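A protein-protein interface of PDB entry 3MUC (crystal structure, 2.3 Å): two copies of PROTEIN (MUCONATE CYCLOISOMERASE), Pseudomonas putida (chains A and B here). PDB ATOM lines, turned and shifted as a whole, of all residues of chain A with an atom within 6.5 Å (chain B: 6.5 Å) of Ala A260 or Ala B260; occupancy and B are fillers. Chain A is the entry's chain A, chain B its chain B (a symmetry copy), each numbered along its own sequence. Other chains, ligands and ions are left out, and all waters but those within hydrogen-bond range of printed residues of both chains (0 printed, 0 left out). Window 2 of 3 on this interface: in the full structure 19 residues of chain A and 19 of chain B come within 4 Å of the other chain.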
ATOM      1  N   ALA A 255      16.488  10.402  10.819  1.00  0.00           N
ATOM      2  CA  ALA A 255      16.219  11.348  11.899  1.00  0.00           C
ATOM      3  C   ALA A 255      14.744  11.737  11.887  1.00  0.00           C
ATOM      4  O   ALA A 255      14.104  11.783  12.933  1.00  0.00           O
ATOM      5  CB  ALA A 255      17.093  12.584  11.744  1.00  0.00           C
ATOM      6  N   PHE A 256      14.206  12.006  10.701  1.00  0.00           N
ATOM      7  CA  PHE A 256      12.805  12.367  10.587  1.00  0.00           C
ATOM      8  C   PHE A 256      11.941  11.204  11.098  1.00  0.00           C
ATOM      9  O   PHE A 256      11.047  11.392  11.942  1.00  0.00           O
ATOM     10  CB  PHE A 256      12.436  12.707   9.144  1.00  0.00           C
ATOM     11  CG  PHE A 256      10.951  12.923   8.952  1.00  0.00           C
ATOM     12  CD1 PHE A 256      10.346  14.106   9.368  1.00  0.00           C
ATOM     13  CD2 PHE A 256      10.140  11.907   8.470  1.00  0.00           C
ATOM     14  CE1 PHE A 256       8.958  14.255   9.314  1.00  0.00           C
ATOM     15  CE2 PHE A 256       8.754  12.060   8.420  1.00  0.00           C
ATOM     16  CZ  PHE A 256       8.168  13.231   8.843  1.00  0.00           C
ATOM     17  N   SER A 257      12.236  10.011  10.582  1.00  0.00           N
ATOM     18  CA  SER A 257      11.547   8.773  10.934  1.00  0.00           C
ATOM     19  C   SER A 257      11.507   8.545  12.455  1.00  0.00           C
ATOM     20  O   SER A 257      10.440   8.343  13.020  1.00  0.00           O
ATOM     21  CB  SER A 257      12.223   7.596  10.210  1.00  0.00           C
ATOM     22  OG  SER A 257      11.492   6.393  10.339  1.00  0.00           O
ATOM     23  N   LEU A 258      12.667   8.594  13.105  1.00  0.00           N
ATOM     24  CA  LEU A 258      12.771   8.414  14.560  1.00  0.00           C
ATOM     25  C   LEU A 258      12.021   9.500  15.318  1.00  0.00           C
ATOM     26  O   LEU A 258      11.455   9.236  16.386  1.00  0.00           O
ATOM     27  CB  LEU A 258      14.230   8.429  15.018  1.00  0.00           C
ATOM     28  CG  LEU A 258      15.095   7.292  14.482  1.00  0.00           C
ATOM     29  CD1 LEU A 258      16.544   7.686  14.577  1.00  0.00           C
ATOM     30  CD2 LEU A 258      14.837   6.006  15.218  1.00  0.00           C
ATOM     31  N   ALA A 259      12.006  10.714  14.771  1.00  0.00           N
ATOM     32  CA  ALA A 259      11.314  11.843  15.390  1.00  0.00           C
ATOM     33  C   ALA A 259       9.813  11.613  15.303  1.00  0.00           C
ATOM     34  O   ALA A 259       9.104  11.698  16.304  1.00  0.00           O
ATOM     35  CB  ALA A 259      11.687  13.166  14.697  1.00  0.00           C
ATOM     36  N   ALA A 260       9.360  11.237  14.114  1.00  0.00           N
ATOM     37  CA  ALA A 260       7.952  11.004  13.874  1.00  0.00           C
ATOM     38  C   ALA A 260       7.453   9.844  14.730  1.00  0.00           C
ATOM     39  O   ALA A 260       6.319   9.859  15.199  1.00  0.00           O
ATOM     40  CB  ALA A 260       7.714  10.752  12.396  1.00  0.00           C
ATOM     41  N   ASP A 261       8.332   8.877  14.982  1.00  0.00           N
ATOM     42  CA  ASP A 261       7.991   7.705  15.779  1.00  0.00           C
ATOM     43  C   ASP A 261       8.078   7.891  17.281  1.00  0.00           C
ATOM     44  O   ASP A 261       7.458   7.141  18.040  1.00  0.00           O
ATOM     45  CB  ASP A 261       8.886   6.518  15.398  1.00  0.00           C
ATOM     46  CG  ASP A 261       8.379   5.742  14.187  1.00  0.00           C
ATOM     47  OD1 ASP A 261       7.369   6.133  13.570  1.00  0.00           O
ATOM     48  OD2 ASP A 261       9.012   4.733  13.838  1.00  0.00           O
ATOM     49  N   GLY A 262       8.880   8.854  17.710  1.00  0.00           N
ATOM     50  CA  GLY A 262       9.083   9.065  19.130  1.00  0.00           C
ATOM     51  C   GLY A 262      10.005   7.961  19.639  1.00  0.00           C
ATOM     52  O   GLY A 262       9.767   7.391  20.705  1.00  0.00           O
ATOM     53  N   ALA A 263      11.055   7.655  18.875  1.00  0.00           N
ATOM     54  CA  ALA A 263      11.996   6.601  19.235  1.00  0.00           C
ATOM     55  C   ALA A 263      13.140   7.023  20.158  1.00  0.00           C
ATOM     56  O   ALA A 263      13.896   6.170  20.634  1.00  0.00           O
ATOM     57  CB  ALA A 263      12.550   5.941  17.975  1.00  0.00           C
ATOM     58  N   ALA A 290      10.823  19.133  16.343  1.00  0.00           N
ATOM     59  CA  ALA A 290      10.091  18.115  17.078  1.00  0.00           C
ATOM     60  C   ALA A 290      10.283  18.228  18.591  1.00  0.00           C
ATOM     61  O   ALA A 290       9.559  17.580  19.346  1.00  0.00           O
ATOM     62  CB  ALA A 290      10.490  16.732  16.593  1.00  0.00           C
ATOM     63  N   ILE A 292      13.275  17.562  20.198  1.00  0.00           N
ATOM     64  CA  ILE A 292      14.239  16.541  20.593  1.00  0.00           C
ATOM     65  C   ILE A 292      15.578  17.209  20.940  1.00  0.00           C
ATOM     66  O   ILE A 292      16.043  18.055  20.192  1.00  0.00           O
ATOM     67  CB  ILE A 292      14.389  15.528  19.446  1.00  0.00           C
ATOM     68  CG1 ILE A 292      13.104  14.711  19.352  1.00  0.00           C
ATOM     69  CG2 ILE A 292      15.644  14.665  19.601  1.00  0.00           C
ATOM     70  CD1 ILE A 292      13.003  13.879  18.114  1.00  0.00           C
ATOM     71  N   ALA B 255       4.946  22.255   9.952  1.00  0.00           N
ATOM     72  CA  ALA B 255       5.370  21.462   8.808  1.00  0.00           C
ATOM     73  C   ALA B 255       5.781  20.065   9.265  1.00  0.00           C
ATOM     74  O   ALA B 255       5.376  19.071   8.660  1.00  0.00           O
ATOM     75  CB  ALA B 255       6.514  22.151   8.097  1.00  0.00           C
ATOM     76  N   PHE B 256       6.536  19.991  10.358  1.00  0.00           N
ATOM     77  CA  PHE B 256       6.951  18.704  10.889  1.00  0.00           C
ATOM     78  C   PHE B 256       5.714  17.877  11.271  1.00  0.00           C
ATOM     79  O   PHE B 256       5.581  16.704  10.879  1.00  0.00           O
ATOM     80  CB  PHE B 256       7.862  18.879  12.107  1.00  0.00           C
ATOM     81  CG  PHE B 256       8.199  17.575  12.789  1.00  0.00           C
ATOM     82  CD1 PHE B 256       9.132  16.699  12.229  1.00  0.00           C
ATOM     83  CD2 PHE B 256       7.501  17.162  13.915  1.00  0.00           C
ATOM     84  CE1 PHE B 256       9.340  15.432  12.781  1.00  0.00           C
ATOM     85  CE2 PHE B 256       7.710  15.901  14.458  1.00  0.00           C
ATOM     86  CZ  PHE B 256       8.626  15.039  13.889  1.00  0.00           C
ATOM     87  N   SER B 257       4.819  18.513  12.024  1.00  0.00           N
ATOM     88  CA  SER B 257       3.572  17.910  12.506  1.00  0.00           C
ATOM     89  C   SER B 257       2.743  17.331  11.347  1.00  0.00           C
ATOM     90  O   SER B 257       2.369  16.168  11.375  1.00  0.00           O
ATOM     91  CB  SER B 257       2.773  18.972  13.296  1.00  0.00           C
ATOM     92  OG  SER B 257       1.652  18.424  13.960  1.00  0.00           O
ATOM     93  N   LEU B 258       2.522  18.132  10.307  1.00  0.00           N
ATOM     94  CA  LEU B 258       1.752  17.702   9.140  1.00  0.00           C
ATOM     95  C   LEU B 258       2.437  16.562   8.426  1.00  0.00           C
ATOM     96  O   LEU B 258       1.769  15.652   7.928  1.00  0.00           O
ATOM     97  CB  LEU B 258       1.536  18.855   8.155  1.00  0.00           C
ATOM     98  CG  LEU B 258       0.676  20.005   8.692  1.00  0.00           C
ATOM     99  CD1 LEU B 258       0.953  21.227   7.878  1.00  0.00           C
ATOM    100  CD2 LEU B 258      -0.807  19.667   8.671  1.00  0.00           C
ATOM    101  N   ALA B 259       3.767  16.597   8.394  1.00  0.00           N
ATOM    102  CA  ALA B 259       4.561  15.555   7.730  1.00  0.00           C
ATOM    103  C   ALA B 259       4.425  14.254   8.501  1.00  0.00           C
ATOM    104  O   ALA B 259       4.066  13.221   7.937  1.00  0.00           O
ATOM    105  CB  ALA B 259       6.039  15.958   7.623  1.00  0.00           C
ATOM    106  N   ALA B 260       4.618  14.342   9.812  1.00  0.00           N
ATOM    107  CA  ALA B 260       4.530  13.178  10.672  1.00  0.00           C
ATOM    108  C   ALA B 260       3.130  12.559  10.601  1.00  0.00           C
ATOM    109  O   ALA B 260       2.980  11.345  10.662  1.00  0.00           O
ATOM    110  CB  ALA B 260       4.897  13.565  12.098  1.00  0.00           C
ATOM    111  N   ASP B 261       2.119  13.402  10.430  1.00  0.00           N
ATOM    112  CA  ASP B 261       0.730  12.953  10.372  1.00  0.00           C
ATOM    113  C   ASP B 261       0.289  12.439   9.019  1.00  0.00           C
ATOM    114  O   ASP B 261      -0.684  11.690   8.926  1.00  0.00           O
ATOM    115  CB  ASP B 261      -0.220  14.093  10.781  1.00  0.00           C
ATOM    116  CG  ASP B 261      -0.421  14.208  12.291  1.00  0.00           C
ATOM    117  OD1 ASP B 261       0.199  13.450  13.069  1.00  0.00           O
ATOM    118  OD2 ASP B 261      -1.210  15.077  12.703  1.00  0.00           O
ATOM    119  N   GLY B 262       0.966  12.881   7.968  1.00  0.00           N
ATOM    120  CA  GLY B 262       0.578  12.500   6.624  1.00  0.00           C
ATOM    121  C   GLY B 262      -0.672  13.288   6.239  1.00  0.00           C
ATOM    122  O   GLY B 262      -1.596  12.740   5.648  1.00  0.00           O
ATOM    123  N   ALA B 263      -0.697  14.573   6.585  1.00  0.00           N
ATOM    124  CA  ALA B 263      -1.840  15.442   6.291  1.00  0.00           C
ATOM    125  C   ALA B 263      -1.866  16.074   4.897  1.00  0.00           C
ATOM    126  O   ALA B 263      -2.848  16.713   4.534  1.00  0.00           O
ATOM    127  CB  ALA B 263      -1.955  16.526   7.358  1.00  0.00           C
ATOM    128  N   ALA B 290      10.824  13.728   4.326  1.00  0.00           N
ATOM    129  CA  ALA B 290       9.618  12.905   4.418  1.00  0.00           C
ATOM    130  C   ALA B 290       9.086  12.474   3.045  1.00  0.00           C
ATOM    131  O   ALA B 290       8.197  11.633   2.976  1.00  0.00           O
ATOM    132  CB  ALA B 290       8.538  13.638   5.185  1.00  0.00           C
ATOM    133  N   ILE B 292       7.749  14.712   0.736  1.00  0.00           N
ATOM    134  CA  ILE B 292       6.627  15.589   0.411  1.00  0.00           C
ATOM    135  C   ILE B 292       7.035  16.587  -0.680  1.00  0.00           C
ATOM    136  O   ILE B 292       8.114  17.162  -0.607  1.00  0.00           O
ATOM    137  CB  ILE B 292       6.148  16.301   1.696  1.00  0.00           C
ATOM    138  CG1 ILE B 292       5.462  15.273   2.594  1.00  0.00           C
ATOM    139  CG2 ILE B 292       5.266  17.494   1.378  1.00  0.00           C
ATOM    140  CD1 ILE B 292       5.223  15.756   3.983  1.00  0.00           C
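Of the 11 printed residues of chain A, 4 touch a printed residue of chain B. Printed residues of chain A that touch a printed residue of chain B: Phe A256, Ala A259, Ala A260 and Ala A290. Along chain A the printed residues that touch a printed residue of chain B span positions 256 to 290. Among the printed residues, 8 pairs touch across the chains. Among the printed residues, no Asp or Glu carboxylate lies within 4 Å of a Lys or Arg side-chain nitrogen of the other chain.
Among the printed residues, pairs that only touch across the chains: Ala A290 with Phe B256, Phe A256 with Ala B290, Phe A256 with Ala B259, Ala A259 with Phe B256, Phe A256 with Phe B256, Phe A256 with Ala B260, Ala A260 with Phe B256 and Ala A260 with Ala B260.
Phe A256 touches Ala B259, and with the chains exchanged Ala A259 touches Phe B256. Phe A256 touches Ala B260, and with the chains exchanged Ala A260 touches Phe B256. Phe A256 touches Ala B290, and with the chains exchanged Ala A290 touches Phe B256. Ala B260 touches its own counterpart, Ala A260. 11 positions are printed for both chains.
Of the printed residues of chain B, Phe A256 touches Phe B256 (3.7 Å), Ala B259 (3.7 Å), Ala B260 (3.8 Å) and Ala B290 (3.6 Å). Ser A257 touches none of the printed residues of chain B. Of the printed residues of chain B, Ala A259 touches Phe B256 (3.7 Å). Printed residues of chain B within 4 Å of Ala A260: Phe B256 (3.9 Å) and Ala B260 (3.99 Å). Asp A261 touches none of the printed residues of chain B. Of the printed residues of chain A, Phe B256 touches Phe A256, Ala A259, Ala A260 and Ala A290. Printed residues of chain A within 4 Å of Ala B259: Phe A256 (3.7 Å). Of the printed residues of chain A, Ala B260 touches Phe A256 and Ala A260. Printed residues of chain A within 4 Å of Ala B290: Phe A256. The nearest printed residue of chain B that does not touch Ala A260 is Ala B259 (6.2 Å). The nearest printed residue of chain A that does not touch Ala B260 is Ala A259 (6.2 Å).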
